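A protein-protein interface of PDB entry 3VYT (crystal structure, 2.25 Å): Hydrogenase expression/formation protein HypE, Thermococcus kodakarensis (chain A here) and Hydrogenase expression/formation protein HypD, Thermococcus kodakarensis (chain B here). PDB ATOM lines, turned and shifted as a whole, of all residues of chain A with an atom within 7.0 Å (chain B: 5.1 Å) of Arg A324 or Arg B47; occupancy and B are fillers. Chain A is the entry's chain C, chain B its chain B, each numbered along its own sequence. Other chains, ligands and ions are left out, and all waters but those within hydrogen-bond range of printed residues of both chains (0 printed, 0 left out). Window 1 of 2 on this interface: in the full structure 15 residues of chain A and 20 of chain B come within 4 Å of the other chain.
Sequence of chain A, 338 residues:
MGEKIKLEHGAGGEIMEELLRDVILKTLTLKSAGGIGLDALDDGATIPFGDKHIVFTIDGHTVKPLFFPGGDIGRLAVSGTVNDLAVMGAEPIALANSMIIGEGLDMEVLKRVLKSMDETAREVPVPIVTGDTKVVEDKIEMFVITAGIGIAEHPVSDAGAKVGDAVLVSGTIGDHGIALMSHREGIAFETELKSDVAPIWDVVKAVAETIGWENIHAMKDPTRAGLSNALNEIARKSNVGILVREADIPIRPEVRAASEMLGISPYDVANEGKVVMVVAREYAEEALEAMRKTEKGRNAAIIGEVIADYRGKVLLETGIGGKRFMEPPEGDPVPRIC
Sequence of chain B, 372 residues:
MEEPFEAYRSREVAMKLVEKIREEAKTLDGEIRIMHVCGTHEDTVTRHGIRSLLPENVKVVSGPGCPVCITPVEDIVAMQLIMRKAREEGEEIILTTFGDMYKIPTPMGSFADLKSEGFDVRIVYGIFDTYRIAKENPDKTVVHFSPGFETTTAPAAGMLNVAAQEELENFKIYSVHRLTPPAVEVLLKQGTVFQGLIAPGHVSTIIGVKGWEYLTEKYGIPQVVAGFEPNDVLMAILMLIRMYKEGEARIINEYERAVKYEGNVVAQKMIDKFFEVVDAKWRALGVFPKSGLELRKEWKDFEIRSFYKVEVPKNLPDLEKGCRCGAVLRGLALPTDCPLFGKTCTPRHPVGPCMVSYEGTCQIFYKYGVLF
Printed residues of chain B that touch a printed residue of chain A: Thr B46, Arg B47, His B48, Gly B49, Tyr B368, Gly B369 and Leu B371. Hydrophobic or aromatic side chains of chain B within 4 Å of the printed part of chain A: Tyr B368 and Leu B371. Of the 19 printed residues of chain A, 7 touch a printed residue of chain B. Hydrophobic or aromatic side chains of chain A within 4 Å of the printed part of chain B: Phe A325. Among the printed residues, 14 pairs touch across the chains. Among the printed residues, Asp or Glu carboxylates within 4 Å of a Lys or Arg side-chain nitrogen of the other chain: Glu A260 with Arg B47.
The guanidinium group (NH1) of Arg B47 lies within salt-bridge range of the side-chain carboxylate (OE2) of Glu A260 (3.0 Å). The backbone carbonyl oxygen (O) of Arg B47 sits at hydrogen-bond distance from the guanidinium group (NE) of Arg A324 (2.9 Å). OG1 of Thr A318 lies within hydrogen-bond range of O of His B48, 2.8 Å away. N of Phe A325 lies within hydrogen-bond range of O of Gly B369 (3.2 Å). O of Phe A325 lies close to O of Tyr B368, at 3.3 Å.
Among the printed residues, pairs that only touch across the chains: Phe A325 with Leu B371 (3.2 Å), Glu A327 with Gly B369 (3.3 Å), Arg A324 with Tyr B368 (3.5 Å), Thr A318 with Arg B47 (3.5 Å), Arg A324 with Thr B46 (3.6 Å), Gly A322 with His B48 (3.7 Å), Gly A322 with Gly B49 (3.7 Å), Lys A323 with Leu B371 (3.8 Å) and Lys A323 with Gly B49 (3.9 Å).
OE2 of Glu B42 sits at hydrogen-bond distance from OG1 of Thr B46. OD1 of Asp B43 lies within salt-bridge range of NH2 of Arg B47. The side-chain carboxylate (OD2) of Asp B43 sits at hydrogen-bond distance from the side-chain hydroxyl (OH) of Tyr B368, 3.2 Å away. NE of Arg B47 lies within hydrogen-bond range of OH of Tyr B368 (3.1 Å). The backbone NH (N) of Leu A316 sits at hydrogen-bond distance from the backbone carbonyl oxygen (O) of Arg A324, 2.5 Å away. The side-chain hydroxyl (OG1) of Thr A318 sits at hydrogen-bond distance from the backbone NH (N) of Gly A322 (2.8 Å).
Arg A324 touches just these residues of chain B: Thr B46 (3.6 Å), Arg B47 (2.9 Å) and Tyr B368 (3.5 Å). Of chain A, only Glu A260 (3.0 Å), Thr A318 (3.5 Å) and Arg A324 (2.9 Å) come within 4 Å of Arg B47. Printed residues of chain B within 4 Å of Glu A260: Arg B47. Of the printed residues of chain A, Tyr B368 touches Arg A324 and Phe A325. Printed residues of chain B within 4 Å of Lys A323: Gly B49 (3.9 Å) and Leu B371 (3.8 Å). Of the printed residues of chain A, Thr B46 touches Arg A324. Tyr A267 touches none of the printed residues of chain B. Thr B44 touches none of the printed residues of chain A. The nearest residue of chain B that does not touch Arg A324 is Gly B369 (4.2 Å).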
ATOM      1  N   LEU A 243     -19.254  -8.186 -12.230  1.00  0.00           N
ATOM      2  CA  LEU A 243     -17.899  -7.673 -12.071  1.00  0.00           C
ATOM      3  C   LEU A 243     -16.904  -8.797 -12.319  1.00  0.00           C
ATOM      4  O   LEU A 243     -16.971  -9.852 -11.694  1.00  0.00           O
ATOM      5  CB  LEU A 243     -17.670  -7.117 -10.665  1.00  0.00           C
ATOM      6  CG  LEU A 243     -16.300  -6.450 -10.514  1.00  0.00           C
ATOM      7  CD1 LEU A 243     -16.268  -5.205 -11.394  1.00  0.00           C
ATOM      8  CD2 LEU A 243     -16.021  -6.092  -9.054  1.00  0.00           C
ATOM      9  N   VAL A 244     -15.982  -8.561 -13.238  1.00  0.00           N
ATOM     10  CA  VAL A 244     -14.970  -9.547 -13.566  1.00  0.00           C
ATOM     11  C   VAL A 244     -13.590  -8.928 -13.377  1.00  0.00           C
ATOM     12  O   VAL A 244     -13.345  -7.792 -13.782  1.00  0.00           O
ATOM     13  CB  VAL A 244     -15.135 -10.039 -15.019  1.00  0.00           C
ATOM     14  CG1 VAL A 244     -13.994 -10.962 -15.393  1.00  0.00           C
ATOM     15  CG2 VAL A 244     -16.446 -10.766 -15.153  1.00  0.00           C
ATOM     16  N   GLU A 246      -9.982  -9.044 -14.453  1.00  0.00           N
ATOM     17  CA  GLU A 246      -9.104  -9.471 -15.532  1.00  0.00           C
ATOM     18  C   GLU A 246      -7.946 -10.344 -15.072  1.00  0.00           C
ATOM     19  O   GLU A 246      -7.560 -11.287 -15.761  1.00  0.00           O
ATOM     20  CB  GLU A 246      -8.567  -8.231 -16.244  1.00  0.00           C
ATOM     21  CG  GLU A 246      -8.033  -8.463 -17.633  1.00  0.00           C
ATOM     22  CD  GLU A 246      -7.716  -7.160 -18.338  1.00  0.00           C
ATOM     23  OE1 GLU A 246      -6.862  -6.406 -17.817  1.00  0.00           O
ATOM     24  OE2 GLU A 246      -8.322  -6.890 -19.403  1.00  0.00           O
ATOM     25  N   GLU A 260      -2.551 -10.953 -29.198  1.00  0.00           N
ATOM     26  CA  GLU A 260      -1.972  -9.630 -29.394  1.00  0.00           C
ATOM     27  C   GLU A 260      -1.525  -9.459 -30.837  1.00  0.00           C
ATOM     28  O   GLU A 260      -1.857  -8.466 -31.480  1.00  0.00           O
ATOM     29  CB  GLU A 260      -0.804  -9.408 -28.435  1.00  0.00           C
ATOM     30  CG  GLU A 260      -1.274  -9.055 -27.040  1.00  0.00           C
ATOM     31  CD  GLU A 260      -2.227  -7.871 -27.053  1.00  0.00           C
ATOM     32  OE1 GLU A 260      -1.775  -6.756 -27.389  1.00  0.00           O
ATOM     33  OE2 GLU A 260      -3.425  -8.062 -26.745  1.00  0.00           O
ATOM     34  N   GLY A 263      -4.273  -9.098 -32.919  1.00  0.00           N
ATOM     35  CA  GLY A 263      -5.034  -7.894 -32.633  1.00  0.00           C
ATOM     36  C   GLY A 263      -6.458  -8.143 -32.163  1.00  0.00           C
ATOM     37  O   GLY A 263      -7.307  -7.264 -32.267  1.00  0.00           O
ATOM     38  N   SER A 265      -9.135  -9.902 -29.006  1.00  0.00           N
ATOM     39  CA  SER A 265      -9.201 -10.231 -27.590  1.00  0.00           C
ATOM     40  C   SER A 265      -9.599 -11.675 -27.369  1.00  0.00           C
ATOM     41  O   SER A 265     -10.530 -12.186 -28.009  1.00  0.00           O
ATOM     42  CB  SER A 265     -10.216  -9.326 -26.877  1.00  0.00           C
ATOM     43  OG  SER A 265     -10.366  -9.688 -25.513  1.00  0.00           O
ATOM     44  N   TYR A 267     -11.202 -12.733 -25.117  1.00  0.00           N
ATOM     45  CA  TYR A 267     -12.515 -12.747 -24.469  1.00  0.00           C
ATOM     46  C   TYR A 267     -13.650 -12.767 -25.480  1.00  0.00           C
ATOM     47  O   TYR A 267     -14.771 -13.133 -25.139  1.00  0.00           O
ATOM     48  CB  TYR A 267     -12.737 -11.513 -23.582  1.00  0.00           C
ATOM     49  CG  TYR A 267     -11.659 -11.207 -22.577  1.00  0.00           C
ATOM     50  CD1 TYR A 267     -10.997 -12.224 -21.897  1.00  0.00           C
ATOM     51  CD2 TYR A 267     -11.324  -9.884 -22.280  1.00  0.00           C
ATOM     52  CE1 TYR A 267     -10.025 -11.933 -20.951  1.00  0.00           C
ATOM     53  CE2 TYR A 267     -10.357  -9.581 -21.335  1.00  0.00           C
ATOM     54  CZ  TYR A 267      -9.710 -10.609 -20.676  1.00  0.00           C
ATOM     55  OH  TYR A 267      -8.737 -10.315 -19.752  1.00  0.00           O
ATOM     56  N   VAL A 314     -21.483  -5.676 -18.131  1.00  0.00           N
ATOM     57  CA  VAL A 314     -20.406  -6.458 -17.548  1.00  0.00           C
ATOM     58  C   VAL A 314     -19.255  -5.505 -17.308  1.00  0.00           C
ATOM     59  O   VAL A 314     -18.713  -4.924 -18.250  1.00  0.00           O
ATOM     60  CB  VAL A 314     -19.953  -7.604 -18.490  1.00  0.00           C
ATOM     61  CG1 VAL A 314     -18.690  -8.265 -17.944  1.00  0.00           C
ATOM     62  CG2 VAL A 314     -21.064  -8.639 -18.609  1.00  0.00           C
ATOM     63  N   LEU A 315     -18.899  -5.342 -16.036  1.00  0.00           N
ATOM     64  CA  LEU A 315     -17.825  -4.441 -15.638  1.00  0.00           C
ATOM     65  C   LEU A 315     -16.519  -5.214 -15.536  1.00  0.00           C
ATOM     66  O   LEU A 315     -16.477  -6.306 -14.971  1.00  0.00           O
ATOM     67  CB  LEU A 315     -18.152  -3.803 -14.285  1.00  0.00           C
ATOM     68  CG  LEU A 315     -17.809  -2.326 -14.097  1.00  0.00           C
ATOM     69  CD1 LEU A 315     -18.702  -1.478 -14.990  1.00  0.00           C
ATOM     70  CD2 LEU A 315     -18.011  -1.944 -12.644  1.00  0.00           C
ATOM     71  N   LEU A 316     -15.455  -4.647 -16.088  1.00  0.00           N
ATOM     72  CA  LEU A 316     -14.157  -5.302 -16.051  1.00  0.00           C
ATOM     73  C   LEU A 316     -13.165  -4.506 -15.222  1.00  0.00           C
ATOM     74  O   LEU A 316     -12.936  -3.325 -15.468  1.00  0.00           O
ATOM     75  CB  LEU A 316     -13.599  -5.472 -17.466  1.00  0.00           C
ATOM     76  CG  LEU A 316     -12.172  -6.029 -17.556  1.00  0.00           C
ATOM     77  CD1 LEU A 316     -12.164  -7.479 -17.097  1.00  0.00           C
ATOM     78  CD2 LEU A 316     -11.656  -5.923 -18.984  1.00  0.00           C
ATOM     79  N   GLU A 317     -12.588  -5.156 -14.224  1.00  0.00           N
ATOM     80  CA  GLU A 317     -11.592  -4.503 -13.400  1.00  0.00           C
ATOM     81  C   GLU A 317     -10.275  -4.931 -14.019  1.00  0.00           C
ATOM     82  O   GLU A 317      -9.922  -6.105 -13.981  1.00  0.00           O
ATOM     83  CB  GLU A 317     -11.685  -4.993 -11.957  1.00  0.00           C
ATOM     84  CG  GLU A 317     -10.679  -4.345 -11.025  1.00  0.00           C
ATOM     85  CD  GLU A 317     -10.846  -4.794  -9.583  1.00  0.00           C
ATOM     86  OE1 GLU A 317      -9.994  -4.428  -8.751  1.00  0.00           O
ATOM     87  OE2 GLU A 317     -11.828  -5.512  -9.281  1.00  0.00           O
ATOM     88  N   THR A 318      -9.553  -3.987 -14.604  1.00  0.00           N
ATOM     89  CA  THR A 318      -8.291  -4.318 -15.244  1.00  0.00           C
ATOM     90  C   THR A 318      -7.183  -4.684 -14.267  1.00  0.00           C
ATOM     91  O   THR A 318      -7.306  -4.481 -13.055  1.00  0.00           O
ATOM     92  CB  THR A 318      -7.807  -3.168 -16.128  1.00  0.00           C
ATOM     93  OG1 THR A 318      -7.571  -2.004 -15.322  1.00  0.00           O
ATOM     94  CG2 THR A 318      -8.853  -2.866 -17.202  1.00  0.00           C
ATOM     95  N   GLY A 319      -6.101  -5.224 -14.818  1.00  0.00           N
ATOM     96  CA  GLY A 319      -4.969  -5.635 -14.017  1.00  0.00           C
ATOM     97  C   GLY A 319      -4.424  -4.554 -13.110  1.00  0.00           C
ATOM     98  O   GLY A 319      -4.154  -4.812 -11.935  1.00  0.00           O
ATOM     99  N   GLY A 322      -7.896  -0.465 -13.032  1.00  0.00           N
ATOM    100  CA  GLY A 322      -8.835   0.424 -13.692  1.00  0.00           C
ATOM    101  C   GLY A 322     -10.185  -0.255 -13.867  1.00  0.00           C
ATOM    102  O   GLY A 322     -10.351  -1.414 -13.474  1.00  0.00           O
ATOM    103  N   LYS A 323     -11.151   0.456 -14.446  1.00  0.00           N
ATOM    104  CA  LYS A 323     -12.480  -0.108 -14.673  1.00  0.00           C
ATOM    105  C   LYS A 323     -12.962   0.241 -16.074  1.00  0.00           C
ATOM    106  O   LYS A 323     -12.741   1.354 -16.557  1.00  0.00           O
ATOM    107  CB  LYS A 323     -13.492   0.443 -13.663  1.00  0.00           C
ATOM    108  CG  LYS A 323     -13.129   0.234 -12.205  1.00  0.00           C
ATOM    109  CD  LYS A 323     -13.436  -1.176 -11.736  1.00  0.00           C
ATOM    110  CE  LYS A 323     -12.900  -1.409 -10.329  1.00  0.00           C
ATOM    111  NZ  LYS A 323     -13.355  -0.371  -9.365  1.00  0.00           N
ATOM    112  N   ARG A 324     -13.602  -0.722 -16.728  1.00  0.00           N
ATOM    113  CA  ARG A 324     -14.161  -0.522 -18.062  1.00  0.00           C
ATOM    114  C   ARG A 324     -15.163  -1.626 -18.315  1.00  0.00           C
ATOM    115  O   ARG A 324     -15.183  -2.621 -17.601  1.00  0.00           O
ATOM    116  CB  ARG A 324     -13.072  -0.537 -19.145  1.00  0.00           C
ATOM    117  CG  ARG A 324     -12.568  -1.901 -19.591  1.00  0.00           C
ATOM    118  CD  ARG A 324     -11.665  -1.715 -20.810  1.00  0.00           C
ATOM    119  NE  ARG A 324     -10.955  -2.928 -21.220  1.00  0.00           N
ATOM    120  CZ  ARG A 324     -11.532  -4.019 -21.715  1.00  0.00           C
ATOM    121  NH1 ARG A 324     -12.845  -4.075 -21.869  1.00  0.00           N
ATOM    122  NH2 ARG A 324     -10.788  -5.056 -22.067  1.00  0.00           N
ATOM    123  N   PHE A 325     -16.013  -1.448 -19.315  1.00  0.00           N
ATOM    124  CA  PHE A 325     -16.993  -2.473 -19.616  1.00  0.00           C
ATOM    125  C   PHE A 325     -16.360  -3.521 -20.508  1.00  0.00           C
ATOM    126  O   PHE A 325     -15.449  -3.217 -21.280  1.00  0.00           O
ATOM    127  CB  PHE A 325     -18.199  -1.882 -20.345  1.00  0.00           C
ATOM    128  CG  PHE A 325     -19.002  -0.931 -19.522  1.00  0.00           C
ATOM    129  CD1 PHE A 325     -19.015   0.428 -19.820  1.00  0.00           C
ATOM    130  CD2 PHE A 325     -19.763  -1.394 -18.458  1.00  0.00           C
ATOM    131  CE1 PHE A 325     -19.782   1.311 -19.068  1.00  0.00           C
ATOM    132  CE2 PHE A 325     -20.530  -0.524 -17.702  1.00  0.00           C
ATOM    133  CZ  PHE A 325     -20.541   0.832 -18.006  1.00  0.00           C
ATOM    134  N   MET A 326     -16.825  -4.757 -20.377  1.00  0.00           N
ATOM    135  CA  MET A 326     -16.348  -5.835 -21.232  1.00  0.00           C
ATOM    136  C   MET A 326     -17.444  -5.921 -22.281  1.00  0.00           C
ATOM    137  O   MET A 326     -18.451  -6.602 -22.099  1.00  0.00           O
ATOM    138  CB  MET A 326     -16.247  -7.157 -20.479  1.00  0.00           C
ATOM    139  CG  MET A 326     -15.692  -8.275 -21.339  1.00  0.00           C
ATOM    140  SD  MET A 326     -15.684  -9.854 -20.499  1.00  0.00           S
ATOM    141  CE  MET A 326     -14.221  -9.662 -19.460  1.00  0.00           C
ATOM    142  N   GLU A 327     -17.247  -5.200 -23.373  1.00  0.00           N
ATOM    143  CA  GLU A 327     -18.228  -5.151 -24.439  1.00  0.00           C
ATOM    144  C   GLU A 327     -18.479  -6.444 -25.196  1.00  0.00           C
ATOM    145  O   GLU A 327     -17.548  -7.160 -25.572  1.00  0.00           O
ATOM    146  CB  GLU A 327     -17.849  -4.048 -25.424  1.00  0.00           C
ATOM    147  CG  GLU A 327     -18.089  -2.652 -24.882  1.00  0.00           C
ATOM    148  CD  GLU A 327     -19.551  -2.424 -24.527  1.00  0.00           C
ATOM    149  OE1 GLU A 327     -20.408  -2.574 -25.427  1.00  0.00           O
ATOM    150  OE2 GLU A 327     -19.843  -2.101 -23.354  1.00  0.00           O
ATOM    151  N   GLU B  42      -3.342   5.147 -27.020  1.00  0.00           N
ATOM    152  CA  GLU B  42      -4.768   5.300 -26.784  1.00  0.00           C
ATOM    153  C   GLU B  42      -5.329   3.944 -26.403  1.00  0.00           C
ATOM    154  O   GLU B  42      -6.213   3.846 -25.541  1.00  0.00           O
ATOM    155  CB  GLU B  42      -5.478   5.816 -28.033  1.00  0.00           C
ATOM    156  CG  GLU B  42      -6.971   6.019 -27.837  1.00  0.00           C
ATOM    157  CD  GLU B  42      -7.285   6.871 -26.618  1.00  0.00           C
ATOM    158  OE1 GLU B  42      -6.592   7.892 -26.396  1.00  0.00           O
ATOM    159  OE2 GLU B  42      -8.234   6.526 -25.885  1.00  0.00           O
ATOM    160  N   ASP B  43      -4.804   2.901 -27.050  1.00  0.00           N
ATOM    161  CA  ASP B  43      -5.235   1.543 -26.771  1.00  0.00           C
ATOM    162  C   ASP B  43      -4.843   1.195 -25.336  1.00  0.00           C
ATOM    163  O   ASP B  43      -5.646   0.643 -24.588  1.00  0.00           O
ATOM    164  CB  ASP B  43      -4.599   0.558 -27.761  1.00  0.00           C
ATOM    165  CG  ASP B  43      -5.048  -0.876 -27.524  1.00  0.00           C
ATOM    166  OD1 ASP B  43      -4.478  -1.556 -26.639  1.00  0.00           O
ATOM    167  OD2 ASP B  43      -5.987  -1.321 -28.209  1.00  0.00           O
ATOM    168  N   THR B  44      -3.613   1.535 -24.954  1.00  0.00           N
ATOM    169  CA  THR B  44      -3.131   1.274 -23.597  1.00  0.00           C
ATOM    170  C   THR B  44      -4.038   2.005 -22.607  1.00  0.00           C
ATOM    171  O   THR B  44      -4.617   1.391 -21.714  1.00  0.00           O
ATOM    172  CB  THR B  44      -1.688   1.793 -23.376  1.00  0.00           C
ATOM    173  OG1 THR B  44      -0.800   1.190 -24.323  1.00  0.00           O
ATOM    174  CG2 THR B  44      -1.218   1.463 -21.969  1.00  0.00           C
ATOM    175  N   VAL B  45      -4.165   3.315 -22.771  1.00  0.00           N
ATOM    176  CA  VAL B  45      -5.004   4.097 -21.873  1.00  0.00           C
ATOM    177  C   VAL B  45      -6.407   3.530 -21.727  1.00  0.00           C
ATOM    178  O   VAL B  45      -6.887   3.336 -20.612  1.00  0.00           O
ATOM    179  CB  VAL B  45      -5.137   5.555 -22.344  1.00  0.00           C
ATOM    180  CG1 VAL B  45      -6.209   6.272 -21.530  1.00  0.00           C
ATOM    181  CG2 VAL B  45      -3.799   6.262 -22.219  1.00  0.00           C
ATOM    182  N   THR B  46      -7.059   3.268 -22.855  1.00  0.00           N
ATOM    183  CA  THR B  46      -8.428   2.759 -22.855  1.00  0.00           C
ATOM    184  C   THR B  46      -8.558   1.306 -22.426  1.00  0.00           C
ATOM    185  O   THR B  46      -9.428   0.972 -21.624  1.00  0.00           O
ATOM    186  CB  THR B  46      -9.078   2.952 -24.246  1.00  0.00           C
ATOM    187  OG1 THR B  46      -9.094   4.352 -24.559  1.00  0.00           O
ATOM    188  CG2 THR B  46     -10.516   2.435 -24.260  1.00  0.00           C
ATOM    189  N   ARG B  47      -7.691   0.445 -22.948  1.00  0.00           N
ATOM    190  CA  ARG B  47      -7.739  -0.974 -22.597  1.00  0.00           C
ATOM    191  C   ARG B  47      -7.594  -1.198 -21.089  1.00  0.00           C
ATOM    192  O   ARG B  47      -8.316  -1.993 -20.504  1.00  0.00           O
ATOM    193  CB  ARG B  47      -6.633  -1.755 -23.319  1.00  0.00           C
ATOM    194  CG  ARG B  47      -6.775  -3.261 -23.159  1.00  0.00           C
ATOM    195  CD  ARG B  47      -5.499  -4.011 -23.467  1.00  0.00           C
ATOM    196  NE  ARG B  47      -5.049  -3.799 -24.833  1.00  0.00           N
ATOM    197  CZ  ARG B  47      -4.254  -4.637 -25.488  1.00  0.00           C
ATOM    198  NH1 ARG B  47      -3.831  -5.746 -24.896  1.00  0.00           N
ATOM    199  NH2 ARG B  47      -3.881  -4.367 -26.733  1.00  0.00           N
ATOM    200  N   HIS B  48      -6.665  -0.488 -20.466  1.00  0.00           N
ATOM    201  CA  HIS B  48      -6.428  -0.643 -19.034  1.00  0.00           C
ATOM    202  C   HIS B  48      -7.279   0.235 -18.126  1.00  0.00           C
ATOM    203  O   HIS B  48      -7.054   0.266 -16.919  1.00  0.00           O
ATOM    204  CB  HIS B  48      -4.948  -0.408 -18.745  1.00  0.00           C
ATOM    205  CG  HIS B  48      -4.051  -1.349 -19.482  1.00  0.00           C
ATOM    206  ND1 HIS B  48      -3.898  -2.668 -19.116  1.00  0.00           N
ATOM    207  CD2 HIS B  48      -3.322  -1.186 -20.610  1.00  0.00           C
ATOM    208  CE1 HIS B  48      -3.114  -3.278 -19.987  1.00  0.00           C
ATOM    209  NE2 HIS B  48      -2.752  -2.400 -20.904  1.00  0.00           N
ATOM    210  N   GLY B  49      -8.251   0.938 -18.702  1.00  0.00           N
ATOM    211  CA  GLY B  49      -9.118   1.808 -17.921  1.00  0.00           C
ATOM    212  C   GLY B  49      -8.383   2.883 -17.142  1.00  0.00           C
ATOM    213  O   GLY B  49      -8.804   3.271 -16.052  1.00  0.00           O
ATOM    214  N   TYR B 368     -13.614  -1.138 -26.540  1.00  0.00           N
ATOM    215  CA  TYR B 368     -13.422  -1.249 -25.091  1.00  0.00           C
ATOM    216  C   TYR B 368     -14.507  -0.720 -24.142  1.00  0.00           C
ATOM    217  O   TYR B 368     -14.285  -0.666 -22.944  1.00  0.00           O
ATOM    218  CB  TYR B 368     -12.077  -0.662 -24.683  1.00  0.00           C
ATOM    219  CG  TYR B 368     -10.898  -1.442 -25.186  1.00  0.00           C
ATOM    220  CD1 TYR B 368      -9.974  -0.861 -26.032  1.00  0.00           C
ATOM    221  CD2 TYR B 368     -10.709  -2.758 -24.821  1.00  0.00           C
ATOM    222  CE1 TYR B 368      -8.899  -1.563 -26.491  1.00  0.00           C
ATOM    223  CE2 TYR B 368      -9.634  -3.467 -25.277  1.00  0.00           C
ATOM    224  CZ  TYR B 368      -8.731  -2.864 -26.111  1.00  0.00           C
ATOM    225  OH  TYR B 368      -7.655  -3.565 -26.572  1.00  0.00           O
ATOM    226  N   GLY B 369     -15.670  -0.329 -24.635  1.00  0.00           N
ATOM    227  CA  GLY B 369     -16.688   0.108 -23.701  1.00  0.00           C
ATOM    228  C   GLY B 369     -16.270   1.182 -22.706  1.00  0.00           C
ATOM    229  O   GLY B 369     -16.245   0.944 -21.501  1.00  0.00           O
ATOM    230  N   LEU B 371     -16.091   4.310 -20.165  1.00  0.00           N
ATOM    231  CA  LEU B 371     -17.003   4.704 -19.095  1.00  0.00           C
ATOM    232  C   LEU B 371     -17.524   6.129 -19.332  1.00  0.00           C
ATOM    233  O   LEU B 371     -17.087   7.058 -18.615  1.00  0.00           O
ATOM    234  CB  LEU B 371     -16.332   4.627 -17.713  1.00  0.00           C
ATOM    235  CG  LEU B 371     -16.181   3.259 -17.032  1.00  0.00           C
ATOM    236  CD1 LEU B 371     -15.799   3.451 -15.569  1.00  0.00           C
ATOM    237  CD2 LEU B 371     -17.484   2.498 -17.110  1.00  0.00           C
